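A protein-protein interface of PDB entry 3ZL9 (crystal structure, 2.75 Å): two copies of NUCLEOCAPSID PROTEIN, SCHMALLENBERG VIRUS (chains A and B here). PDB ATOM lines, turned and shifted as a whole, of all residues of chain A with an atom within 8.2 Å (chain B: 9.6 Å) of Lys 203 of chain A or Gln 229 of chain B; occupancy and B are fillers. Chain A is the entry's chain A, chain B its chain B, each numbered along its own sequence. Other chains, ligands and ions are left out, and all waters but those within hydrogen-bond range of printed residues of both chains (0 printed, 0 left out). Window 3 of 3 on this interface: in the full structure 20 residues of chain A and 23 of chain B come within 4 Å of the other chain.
The side-chain sulfur (SD) of Met 195 of chain A lies close to the backbone NH (N) of Ala 223 of chain B (3.8 Å).
SD of Met 195 of chain A sits close to O of Ala 222 of chain B (3.7 Å).
The side-chain amide oxygen (OD1) of Asn 207 of chain A sits close to the backbone carbonyl oxygen (O) of Lys 203 of chain A (3.0 Å).
The backbone carbonyl oxygen (O) of Leu 227 of chain B lies within hydrogen-bond range of the backbone NH (N) of Ile 232 of chain B (3.2 Å).
Among the printed residues, merely in contact across the chains: Leu 161 of chain A with Phe 226 of chain B (3.8 Å), Met 165 of chain A with Phe 226 of chain B (3.9 Å), Met 165 of chain A with Leu 227 of chain B (3.3 Å), Met 165 of chain A with Phe 230 of chain B (3.7 Å), Met 165 of chain A with Ile 232 of chain B (3.8 Å), Leu 169 of chain A with Phe 230 of chain B (3.7 Å), Leu 169 of chain A with Gly 231 of chain B (3.7 Å), Leu 169 of chain A with Ile 232 of chain B (3.7 Å), Met 195 of chain A with Phe 226 of chain B (3.7 Å), Ile 199 of chain A with Gln 229 of chain B (3.5 Å), Ile 202 of chain A with Phe 226 of chain B (3.8 Å), Ile 202 of chain A with Phe 230 of chain B (3.4 Å), Lys 203 of chain A with Gln 229 of chain B (3.5 Å), Lys 203 of chain A with Phe 230 of chain B (3.5 Å) and Phe 206 of chain A with Phe 230 of chain B (3.5 Å).
Phe 158 of chain A touches none of the printed residues of chain B.
Of the printed residues of chain B, Leu 161 of chain A touches Phe 226.
Of the printed residues of chain B, Met 165 of chain A touches Phe 226, Leu 227, Phe 230 and Ile 232.
Of the printed residues of chain B, Ile 199 of chain A touches Gln 229 (3.5 Å).
No residue of chain B comes within 4 Å of Ala 204 of chain A.
No residue of chain B comes within 4 Å of Ala 205 of chain A.
Asn 207 of chain A touches none of the printed residues of chain B.
Of the printed residues of chain A, Gln 229 of chain B touches Ile 199 and Lys 203.
Of the printed residues of chain A, Gly 231 of chain B touches Leu 169 (3.7 Å).
The nearest residue of chain A that does not touch Gln 229 of chain B is Met 195 of chain A (4.4 Å).
Of the 23 printed residues of chain A, 8 touch a printed residue of chain B.
Of the 13 printed residues of chain B, 8 touch a printed residue of chain A.
Hydrophobic or aromatic side chains of chain B that line the printed part of chain A: Ala 223, Phe 226, Leu 227, Phe 230 and Ile 232.
Among the printed residues, 17 pairs touch across the chains.
No position is printed for both chains.
Of the 17 pairs that touch across the chains among the printed residues, none has its exchanged pair printed and touching as well.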
ATOM      1  N   PHE A 158      27.660 -22.081 -17.783  1.00  0.00           N
ATOM      2  CA  PHE A 158      26.568 -22.239 -16.799  1.00  0.00           C
ATOM      3  C   PHE A 158      25.160 -22.110 -17.372  1.00  0.00           C
ATOM      4  O   PHE A 158      24.194 -22.324 -16.646  1.00  0.00           O
ATOM      5  CB  PHE A 158      26.712 -21.252 -15.638  1.00  0.00           C
ATOM      6  CG  PHE A 158      27.860 -21.553 -14.739  1.00  0.00           C
ATOM      7  CD1 PHE A 158      27.846 -22.674 -13.932  1.00  0.00           C
ATOM      8  CD2 PHE A 158      28.952 -20.726 -14.694  1.00  0.00           C
ATOM      9  CE1 PHE A 158      28.905 -22.961 -13.105  1.00  0.00           C
ATOM     10  CE2 PHE A 158      30.016 -21.007 -13.845  1.00  0.00           C
ATOM     11  CZ  PHE A 158      29.981 -22.126 -13.050  1.00  0.00           C
ATOM     12  N   LEU A 161      22.621 -24.861 -16.638  1.00  0.00           N
ATOM     13  CA  LEU A 161      22.176 -24.885 -15.238  1.00  0.00           C
ATOM     14  C   LEU A 161      21.074 -23.870 -15.014  1.00  0.00           C
ATOM     15  O   LEU A 161      20.021 -24.199 -14.479  1.00  0.00           O
ATOM     16  CB  LEU A 161      23.341 -24.589 -14.290  1.00  0.00           C
ATOM     17  CG  LEU A 161      23.020 -24.150 -12.856  1.00  0.00           C
ATOM     18  CD1 LEU A 161      22.266 -25.241 -12.124  1.00  0.00           C
ATOM     19  CD2 LEU A 161      24.296 -23.796 -12.112  1.00  0.00           C
ATOM     20  N   VAL A 162      21.336 -22.623 -15.395  1.00  0.00           N
ATOM     21  CA  VAL A 162      20.370 -21.544 -15.200  1.00  0.00           C
ATOM     22  C   VAL A 162      19.123 -21.721 -16.059  1.00  0.00           C
ATOM     23  O   VAL A 162      18.041 -21.323 -15.672  1.00  0.00           O
ATOM     24  CB  VAL A 162      20.993 -20.168 -15.472  1.00  0.00           C
ATOM     25  CG1 VAL A 162      22.147 -19.910 -14.516  1.00  0.00           C
ATOM     26  CG2 VAL A 162      21.468 -20.057 -16.916  1.00  0.00           C
ATOM     27  N   MET A 165      16.977 -23.732 -14.160  1.00  0.00           N
ATOM     28  CA  MET A 165      16.453 -22.993 -13.007  1.00  0.00           C
ATOM     29  C   MET A 165      15.206 -22.219 -13.404  1.00  0.00           C
ATOM     30  O   MET A 165      14.256 -22.073 -12.624  1.00  0.00           O
ATOM     31  CB  MET A 165      17.519 -22.055 -12.414  1.00  0.00           C
ATOM     32  CG  MET A 165      18.772 -22.778 -11.913  1.00  0.00           C
ATOM     33  SD  MET A 165      19.814 -21.804 -10.804  1.00  0.00           S
ATOM     34  CE  MET A 165      18.725 -21.851  -9.388  1.00  0.00           C
ATOM     35  N   HIS A 166      15.220 -21.703 -14.630  1.00  0.00           N
ATOM     36  CA  HIS A 166      14.081 -20.964 -15.146  1.00  0.00           C
ATOM     37  C   HIS A 166      12.873 -21.845 -15.433  1.00  0.00           C
ATOM     38  O   HIS A 166      11.734 -21.419 -15.222  1.00  0.00           O
ATOM     39  CB  HIS A 166      14.467 -20.167 -16.383  1.00  0.00           C
ATOM     40  CG  HIS A 166      15.096 -18.851 -16.063  1.00  0.00           C
ATOM     41  ND1 HIS A 166      16.445 -18.616 -16.208  1.00  0.00           N
ATOM     42  CD2 HIS A 166      14.566 -17.712 -15.552  1.00  0.00           C
ATOM     43  CE1 HIS A 166      16.716 -17.376 -15.830  1.00  0.00           C
ATOM     44  NE2 HIS A 166      15.594 -16.806 -15.424  1.00  0.00           N
ATOM     45  N   LEU A 169      11.108 -22.277 -12.299  1.00  0.00           N
ATOM     46  CA  LEU A 169      10.499 -20.997 -11.888  1.00  0.00           C
ATOM     47  C   LEU A 169       9.327 -20.606 -12.764  1.00  0.00           C
ATOM     48  O   LEU A 169       8.217 -20.434 -12.285  1.00  0.00           O
ATOM     49  CB  LEU A 169      11.544 -19.867 -11.858  1.00  0.00           C
ATOM     50  CG  LEU A 169      12.508 -19.927 -10.658  1.00  0.00           C
ATOM     51  CD1 LEU A 169      13.603 -18.874 -10.733  1.00  0.00           C
ATOM     52  CD2 LEU A 169      11.756 -19.804  -9.334  1.00  0.00           C
ATOM     53  N   TRP A 194      31.726 -24.570  -6.825  1.00  0.00           N
ATOM     54  CA  TRP A 194      31.286 -23.494  -7.709  1.00  0.00           C
ATOM     55  C   TRP A 194      29.975 -22.869  -7.297  1.00  0.00           C
ATOM     56  O   TRP A 194      29.688 -21.729  -7.668  1.00  0.00           O
ATOM     57  CB  TRP A 194      31.232 -23.889  -9.201  1.00  0.00           C
ATOM     58  CG  TRP A 194      30.415 -25.106  -9.585  1.00  0.00           C
ATOM     59  CD1 TRP A 194      30.906 -26.329  -9.922  1.00  0.00           C
ATOM     60  CD2 TRP A 194      28.986 -25.192  -9.733  1.00  0.00           C
ATOM     61  NE1 TRP A 194      29.874 -27.183 -10.260  1.00  0.00           N
ATOM     62  CE2 TRP A 194      28.688 -26.505 -10.165  1.00  0.00           C
ATOM     63  CE3 TRP A 194      27.932 -24.295  -9.531  1.00  0.00           C
ATOM     64  CZ2 TRP A 194      27.381 -26.952 -10.366  1.00  0.00           C
ATOM     65  CZ3 TRP A 194      26.618 -24.732  -9.766  1.00  0.00           C
ATOM     66  CH2 TRP A 194      26.358 -26.053 -10.161  1.00  0.00           C
ATOM     67  N   MET A 195      29.172 -23.584  -6.531  1.00  0.00           N
ATOM     68  CA  MET A 195      28.004 -22.948  -5.937  1.00  0.00           C
ATOM     69  C   MET A 195      28.405 -21.711  -5.112  1.00  0.00           C
ATOM     70  O   MET A 195      27.595 -20.807  -4.905  1.00  0.00           O
ATOM     71  CB  MET A 195      27.210 -23.953  -5.088  1.00  0.00           C
ATOM     72  CG  MET A 195      26.392 -24.912  -5.935  1.00  0.00           C
ATOM     73  SD  MET A 195      25.797 -26.392  -5.074  1.00  0.00           S
ATOM     74  CE  MET A 195      24.810 -27.124  -6.355  1.00  0.00           C
ATOM     75  N   THR A 196      29.649 -21.690  -4.638  1.00  0.00           N
ATOM     76  CA  THR A 196      30.185 -20.584  -3.848  1.00  0.00           C
ATOM     77  C   THR A 196      30.970 -19.612  -4.718  1.00  0.00           C
ATOM     78  O   THR A 196      30.640 -18.426  -4.813  1.00  0.00           O
ATOM     79  CB  THR A 196      31.150 -21.107  -2.762  1.00  0.00           C
ATOM     80  OG1 THR A 196      30.413 -21.833  -1.776  1.00  0.00           O
ATOM     81  CG2 THR A 196      31.891 -19.955  -2.091  1.00  0.00           C
ATOM     82  N   GLN A 197      32.023 -20.128  -5.340  1.00  0.00           N
ATOM     83  CA  GLN A 197      33.032 -19.283  -5.971  1.00  0.00           C
ATOM     84  C   GLN A 197      32.582 -18.697  -7.296  1.00  0.00           C
ATOM     85  O   GLN A 197      33.258 -17.807  -7.829  1.00  0.00           O
ATOM     86  CB  GLN A 197      34.337 -20.060  -6.173  1.00  0.00           C
ATOM     87  CG  GLN A 197      34.936 -20.604  -4.878  1.00  0.00           C
ATOM     88  CD  GLN A 197      36.193 -21.421  -5.101  1.00  0.00           C
ATOM     89  OE1 GLN A 197      37.081 -21.027  -5.865  1.00  0.00           O
ATOM     90  NE2 GLN A 197      36.276 -22.566  -4.436  1.00  0.00           N
ATOM     91  N   LYS A 198      31.436 -19.159  -7.803  1.00  0.00           N
ATOM     92  CA  LYS A 198      30.968 -18.763  -9.122  1.00  0.00           C
ATOM     93  C   LYS A 198      29.579 -18.128  -9.158  1.00  0.00           C
ATOM     94  O   LYS A 198      29.024 -17.961 -10.235  1.00  0.00           O
ATOM     95  CB  LYS A 198      31.035 -19.982 -10.047  1.00  0.00           C
ATOM     96  CG  LYS A 198      32.453 -20.490 -10.279  1.00  0.00           C
ATOM     97  CD  LYS A 198      33.291 -19.416 -10.969  1.00  0.00           C
ATOM     98  CE  LYS A 198      34.546 -19.977 -11.609  1.00  0.00           C
ATOM     99  NZ  LYS A 198      35.044 -19.056 -12.673  1.00  0.00           N
ATOM    100  N   ILE A 199      29.014 -17.756  -8.013  1.00  0.00           N
ATOM    101  CA  ILE A 199      27.683 -17.117  -8.011  1.00  0.00           C
ATOM    102  C   ILE A 199      27.599 -15.827  -8.823  1.00  0.00           C
ATOM    103  O   ILE A 199      26.512 -15.464  -9.274  1.00  0.00           O
ATOM    104  CB  ILE A 199      27.129 -16.806  -6.595  1.00  0.00           C
ATOM    105  CG1 ILE A 199      28.255 -16.422  -5.625  1.00  0.00           C
ATOM    106  CG2 ILE A 199      26.316 -17.991  -6.066  1.00  0.00           C
ATOM    107  CD1 ILE A 199      27.785 -15.667  -4.392  1.00  0.00           C
ATOM    108  N   THR A 200      28.715 -15.118  -8.981  1.00  0.00           N
ATOM    109  CA  THR A 200      28.700 -13.852  -9.716  1.00  0.00           C
ATOM    110  C   THR A 200      28.443 -14.111 -11.186  1.00  0.00           C
ATOM    111  O   THR A 200      27.502 -13.554 -11.752  1.00  0.00           O
ATOM    112  CB  THR A 200      29.995 -13.040  -9.535  1.00  0.00           C
ATOM    113  OG1 THR A 200      31.131 -13.878  -9.778  1.00  0.00           O
ATOM    114  CG2 THR A 200      30.076 -12.475  -8.121  1.00  0.00           C
ATOM    115  N   GLU A 201      29.250 -14.982 -11.794  1.00  0.00           N
ATOM    116  CA  GLU A 201      29.030 -15.353 -13.214  1.00  0.00           C
ATOM    117  C   GLU A 201      27.750 -16.170 -13.426  1.00  0.00           C
ATOM    118  O   GLU A 201      27.165 -16.097 -14.492  1.00  0.00           O
ATOM    119  CB  GLU A 201      30.238 -16.061 -13.868  1.00  0.00           C
ATOM    120  CG  GLU A 201      31.090 -16.949 -12.975  1.00  0.00           C
ATOM    121  CD  GLU A 201      32.268 -16.209 -12.356  1.00  0.00           C
ATOM    122  OE1 GLU A 201      33.217 -15.889 -13.104  1.00  0.00           O
ATOM    123  OE2 GLU A 201      32.246 -15.950 -11.127  1.00  0.00           O
ATOM    124  N   ILE A 202      27.312 -16.913 -12.401  1.00  0.00           N
ATOM    125  CA  ILE A 202      26.053 -17.659 -12.476  1.00  0.00           C
ATOM    126  C   ILE A 202      24.840 -16.722 -12.470  1.00  0.00           C
ATOM    127  O   ILE A 202      23.961 -16.830 -13.330  1.00  0.00           O
ATOM    128  CB  ILE A 202      25.918 -18.693 -11.348  1.00  0.00           C
ATOM    129  CG1 ILE A 202      26.905 -19.848 -11.567  1.00  0.00           C
ATOM    130  CG2 ILE A 202      24.493 -19.259 -11.298  1.00  0.00           C
ATOM    131  CD1 ILE A 202      27.137 -20.703 -10.337  1.00  0.00           C
ATOM    132  N   LYS A 203      24.797 -15.783 -11.531  1.00  0.00           N
ATOM    133  CA  LYS A 203      23.725 -14.786 -11.541  1.00  0.00           C
ATOM    134  C   LYS A 203      23.715 -13.994 -12.849  1.00  0.00           C
ATOM    135  O   LYS A 203      22.637 -13.609 -13.309  1.00  0.00           O
ATOM    136  CB  LYS A 203      23.803 -13.841 -10.337  1.00  0.00           C
ATOM    137  CG  LYS A 203      23.285 -14.489  -9.071  1.00  0.00           C
ATOM    138  CD  LYS A 203      23.175 -13.520  -7.906  1.00  0.00           C
ATOM    139  CE  LYS A 203      22.924 -14.274  -6.608  1.00  0.00           C
ATOM    140  NZ  LYS A 203      22.869 -13.373  -5.428  1.00  0.00           N
ATOM    141  N   ALA A 204      24.894 -13.777 -13.444  1.00  0.00           N
ATOM    142  CA  ALA A 204      24.976 -13.056 -14.719  1.00  0.00           C
ATOM    143  C   ALA A 204      24.322 -13.872 -15.830  1.00  0.00           C
ATOM    144  O   ALA A 204      23.432 -13.366 -16.529  1.00  0.00           O
ATOM    145  CB  ALA A 204      26.419 -12.720 -15.078  1.00  0.00           C
ATOM    146  N   ALA A 205      24.720 -15.135 -15.960  1.00  0.00           N
ATOM    147  CA  ALA A 205      24.076 -16.038 -16.925  1.00  0.00           C
ATOM    148  C   ALA A 205      22.572 -16.177 -16.662  1.00  0.00           C
ATOM    149  O   ALA A 205      21.751 -16.111 -17.577  1.00  0.00           O
ATOM    150  CB  ALA A 205      24.743 -17.404 -16.893  1.00  0.00           C
ATOM    151  N   PHE A 206      22.208 -16.349 -15.395  1.00  0.00           N
ATOM    152  CA  PHE A 206      20.808 -16.413 -15.009  1.00  0.00           C
ATOM    153  C   PHE A 206      20.058 -15.172 -15.492  1.00  0.00           C
ATOM    154  O   PHE A 206      19.003 -15.281 -16.108  1.00  0.00           O
ATOM    155  CB  PHE A 206      20.683 -16.533 -13.490  1.00  0.00           C
ATOM    156  CG  PHE A 206      19.262 -16.694 -13.011  1.00  0.00           C
ATOM    157  CD1 PHE A 206      18.665 -17.936 -12.967  1.00  0.00           C
ATOM    158  CD2 PHE A 206      18.529 -15.587 -12.604  1.00  0.00           C
ATOM    159  CE1 PHE A 206      17.363 -18.083 -12.513  1.00  0.00           C
ATOM    160  CE2 PHE A 206      17.222 -15.725 -12.152  1.00  0.00           C
ATOM    161  CZ  PHE A 206      16.638 -16.973 -12.105  1.00  0.00           C
ATOM    162  N   ASN A 207      20.600 -13.992 -15.197  1.00  0.00           N
ATOM    163  CA  ASN A 207      19.984 -12.723 -15.638  1.00  0.00           C
ATOM    164  C   ASN A 207      19.877 -12.607 -17.157  1.00  0.00           C
ATOM    165  O   ASN A 207      18.893 -12.077 -17.655  1.00  0.00           O
ATOM    166  CB  ASN A 207      20.752 -11.502 -15.102  1.00  0.00           C
ATOM    167  CG  ASN A 207      20.718 -11.388 -13.580  1.00  0.00           C
ATOM    168  OD1 ASN A 207      21.644 -10.837 -12.979  1.00  0.00           O
ATOM    169  ND2 ASN A 207      19.671 -11.926 -12.947  1.00  0.00           N
ATOM    170  N   SER A 208      20.870 -13.134 -17.877  1.00  0.00           N
ATOM    171  CA  SER A 208      20.902 -13.054 -19.344  1.00  0.00           C
ATOM    172  C   SER A 208      19.786 -13.865 -19.999  1.00  0.00           C
ATOM    173  O   SER A 208      19.087 -13.346 -20.869  1.00  0.00           O
ATOM    174  CB  SER A 208      22.236 -13.557 -19.901  1.00  0.00           C
ATOM    175  OG  SER A 208      23.294 -12.646 -19.655  1.00  0.00           O
ATOM    176  N   VAL A 209      19.612 -15.126 -19.593  1.00  0.00           N
ATOM    177  CA  VAL A 209      18.536 -15.940 -20.173  1.00  0.00           C
ATOM    178  C   VAL A 209      17.192 -15.442 -19.680  1.00  0.00           C
ATOM    179  O   VAL A 209      16.171 -15.588 -20.348  1.00  0.00           O
ATOM    180  CB  VAL A 209      18.684 -17.451 -19.897  1.00  0.00           C
ATOM    181  CG1 VAL A 209      20.120 -17.899 -20.089  1.00  0.00           C
ATOM    182  CG2 VAL A 209      18.238 -17.808 -18.506  1.00  0.00           C
ATOM    183  N   GLY A 210      17.205 -14.813 -18.504  1.00  0.00           N
ATOM    184  CA  GLY A 210      16.011 -14.178 -17.954  1.00  0.00           C
ATOM    185  C   GLY A 210      15.465 -13.034 -18.794  1.00  0.00           C
ATOM    186  O   GLY A 210      14.378 -12.531 -18.516  1.00  0.00           O
ATOM    187  N   PRO B 221      23.236 -29.807   1.417  1.00  0.00           N
ATOM    188  CA  PRO B 221      22.943 -28.508   2.027  1.00  0.00           C
ATOM    189  C   PRO B 221      23.423 -27.325   1.180  1.00  0.00           C
ATOM    190  O   PRO B 221      22.695 -26.335   1.044  1.00  0.00           O
ATOM    191  CB  PRO B 221      23.692 -28.562   3.370  1.00  0.00           C
ATOM    192  CG  PRO B 221      24.485 -29.842   3.372  1.00  0.00           C
ATOM    193  CD  PRO B 221      23.835 -30.751   2.378  1.00  0.00           C
ATOM    194  N   ALA B 222      24.614 -27.448   0.595  1.00  0.00           N
ATOM    195  CA  ALA B 222      25.200 -26.393  -0.253  1.00  0.00           C
ATOM    196  C   ALA B 222      24.377 -26.114  -1.499  1.00  0.00           C
ATOM    197  O   ALA B 222      24.355 -24.987  -2.004  1.00  0.00           O
ATOM    198  CB  ALA B 222      26.614 -26.770  -0.656  1.00  0.00           C
ATOM    199  N   ALA B 223      23.718 -27.151  -2.001  1.00  0.00           N
ATOM    200  CA  ALA B 223      22.836 -27.017  -3.152  1.00  0.00           C
ATOM    201  C   ALA B 223      21.575 -26.240  -2.792  1.00  0.00           C
ATOM    202  O   ALA B 223      21.025 -25.524  -3.622  1.00  0.00           O
ATOM    203  CB  ALA B 223      22.465 -28.393  -3.685  1.00  0.00           C
ATOM    204  N   ARG B 224      21.097 -26.392  -1.562  1.00  0.00           N
ATOM    205  CA  ARG B 224      19.858 -25.722  -1.142  1.00  0.00           C
ATOM    206  C   ARG B 224      20.120 -24.237  -0.963  1.00  0.00           C
ATOM    207  O   ARG B 224      19.328 -23.399  -1.420  1.00  0.00           O
ATOM    208  CB  ARG B 224      19.351 -26.301   0.152  1.00  0.00           C
ATOM    209  CG  ARG B 224      18.165 -27.255   0.052  1.00  0.00           C
ATOM    210  CD  ARG B 224      18.067 -28.070   1.359  1.00  0.00           C
ATOM    211  NE  ARG B 224      18.998 -29.201   1.368  1.00  0.00           N
ATOM    212  CZ  ARG B 224      19.411 -29.843   2.461  1.00  0.00           C
ATOM    213  NH1 ARG B 224      19.017 -29.465   3.679  1.00  0.00           N
ATOM    214  NH2 ARG B 224      20.246 -30.869   2.347  1.00  0.00           N
ATOM    215  N   THR B 225      21.259 -23.923  -0.338  1.00  0.00           N
ATOM    216  CA  THR B 225      21.710 -22.547  -0.163  1.00  0.00           C
ATOM    217  C   THR B 225      21.871 -21.871  -1.515  1.00  0.00           C
ATOM    218  O   THR B 225      21.469 -20.723  -1.702  1.00  0.00           O
ATOM    219  CB  THR B 225      23.078 -22.487   0.542  1.00  0.00           C
ATOM    220  OG1 THR B 225      23.022 -23.195   1.776  1.00  0.00           O
ATOM    221  CG2 THR B 225      23.504 -21.029   0.792  1.00  0.00           C
ATOM    222  N   PHE B 226      22.486 -22.591  -2.447  1.00  0.00           N
ATOM    223  CA  PHE B 226      22.686 -22.094  -3.796  1.00  0.00           C
ATOM    224  C   PHE B 226      21.373 -21.669  -4.452  1.00  0.00           C
ATOM    225  O   PHE B 226      21.241 -20.526  -4.901  1.00  0.00           O
ATOM    226  CB  PHE B 226      23.354 -23.160  -4.655  1.00  0.00           C
ATOM    227  CG  PHE B 226      23.395 -22.801  -6.107  1.00  0.00           C
ATOM    228  CD1 PHE B 226      24.229 -21.790  -6.556  1.00  0.00           C
ATOM    229  CD2 PHE B 226      22.569 -23.432  -7.025  1.00  0.00           C
ATOM    230  CE1 PHE B 226      24.264 -21.441  -7.899  1.00  0.00           C
ATOM    231  CE2 PHE B 226      22.596 -23.071  -8.363  1.00  0.00           C
ATOM    232  CZ  PHE B 226      23.447 -22.078  -8.801  1.00  0.00           C
ATOM    233  N   LEU B 227      20.419 -22.594  -4.513  1.00  0.00           N
ATOM    234  CA  LEU B 227      19.132 -22.325  -5.149  1.00  0.00           C
ATOM    235  C   LEU B 227      18.367 -21.173  -4.484  1.00  0.00           C
ATOM    236  O   LEU B 227      17.776 -20.358  -5.185  1.00  0.00           O
ATOM    237  CB  LEU B 227      18.262 -23.555  -5.127  1.00  0.00           C
ATOM    238  CG  LEU B 227      18.693 -24.775  -5.945  1.00  0.00           C
ATOM    239  CD1 LEU B 227      17.812 -25.979  -5.620  1.00  0.00           C
ATOM    240  CD2 LEU B 227      18.662 -24.490  -7.436  1.00  0.00           C
ATOM    241  N   GLN B 228      18.408 -21.084  -3.155  1.00  0.00           N
ATOM    242  CA  GLN B 228      17.803 -19.962  -2.431  1.00  0.00           C
ATOM    243  C   GLN B 228      18.155 -18.615  -3.046  1.00  0.00           C
ATOM    244  O   GLN B 228      17.304 -17.738  -3.148  1.00  0.00           O
ATOM    245  CB  GLN B 228      18.248 -19.929  -0.968  1.00  0.00           C
ATOM    246  CG  GLN B 228      17.467 -20.867  -0.070  1.00  0.00           C
ATOM    247  CD  GLN B 228      17.919 -20.809   1.377  1.00  0.00           C
ATOM    248  OE1 GLN B 228      18.568 -19.847   1.806  1.00  0.00           O
ATOM    249  NE2 GLN B 228      17.565 -21.834   2.148  1.00  0.00           N
ATOM    250  N   GLN B 229      19.407 -18.464  -3.469  1.00  0.00           N
ATOM    251  CA  GLN B 229      19.888 -17.205  -4.041  1.00  0.00           C
ATOM    252  C   GLN B 229      19.141 -16.789  -5.300  1.00  0.00           C
ATOM    253  O   GLN B 229      19.144 -15.624  -5.672  1.00  0.00           O
ATOM    254  CB  GLN B 229      21.387 -17.301  -4.328  1.00  0.00           C
ATOM    255  CG  GLN B 229      22.194 -17.580  -3.065  1.00  0.00           C
ATOM    256  CD  GLN B 229      23.678 -17.349  -3.247  1.00  0.00           C
ATOM    257  OE1 GLN B 229      24.473 -18.278  -3.129  1.00  0.00           O
ATOM    258  NE2 GLN B 229      24.062 -16.104  -3.546  1.00  0.00           N
ATOM    259  N   PHE B 230      18.498 -17.750  -5.953  1.00  0.00           N
ATOM    260  CA  PHE B 230      17.680 -17.491  -7.133  1.00  0.00           C
ATOM    261  C   PHE B 230      16.203 -17.679  -6.806  1.00  0.00           C
ATOM    262  O   PHE B 230      15.361 -17.773  -7.703  1.00  0.00           O
ATOM    263  CB  PHE B 230      18.133 -18.406  -8.263  1.00  0.00           C
ATOM    264  CG  PHE B 230      19.565 -18.225  -8.606  1.00  0.00           C
ATOM    265  CD1 PHE B 230      20.546 -18.857  -7.873  1.00  0.00           C
ATOM    266  CD2 PHE B 230      19.938 -17.364  -9.626  1.00  0.00           C
ATOM    267  CE1 PHE B 230      21.878 -18.663  -8.168  1.00  0.00           C
ATOM    268  CE2 PHE B 230      21.269 -17.165  -9.928  1.00  0.00           C
ATOM    269  CZ  PHE B 230      22.242 -17.813  -9.192  1.00  0.00           C
ATOM    270  N   GLY B 231      15.897 -17.706  -5.511  1.00  0.00           N
ATOM    271  CA  GLY B 231      14.532 -17.758  -5.045  1.00  0.00           C
ATOM    272  C   GLY B 231      13.888 -19.084  -5.336  1.00  0.00           C
ATOM    273  O   GLY B 231      12.757 -19.141  -5.796  1.00  0.00           O
ATOM    274  N   ILE B 232      14.623 -20.155  -5.102  1.00  0.00           N
ATOM    275  CA  ILE B 232      14.076 -21.498  -5.215  1.00  0.00           C
ATOM    276  C   ILE B 232      14.258 -22.194  -3.872  1.00  0.00           C
ATOM    277  O   ILE B 232      15.380 -22.347  -3.376  1.00  0.00           O
ATOM    278  CB  ILE B 232      14.745 -22.294  -6.344  1.00  0.00           C
ATOM    279  CG1 ILE B 232      14.588 -21.539  -7.654  1.00  0.00           C
ATOM    280  CG2 ILE B 232      14.134 -23.689  -6.445  1.00  0.00           C
ATOM    281  CD1 ILE B 232      14.922 -22.342  -8.892  1.00  0.00           C
ATOM    282  N   ASN B 233      13.133 -22.586  -3.283  1.00  0.00           N
ATOM    283  CA  ASN B 233      13.128 -23.204  -1.972  1.00  0.00           C
ATOM    284  C   ASN B 233      12.627 -24.620  -2.035  1.00  0.00           C
ATOM    285  O   ASN B 233      11.783 -24.952  -2.859  1.00  0.00           O
ATOM    286  CB  ASN B 233      12.265 -22.386  -1.028  1.00  0.00           C
ATOM    287  CG  ASN B 233      12.760 -20.960  -0.897  1.00  0.00           C
ATOM    288  OD1 ASN B 233      12.040 -20.010  -1.212  1.00  0.00           O
ATOM    289  ND2 ASN B 233      14.000 -20.805  -0.457  1.00  0.00           N
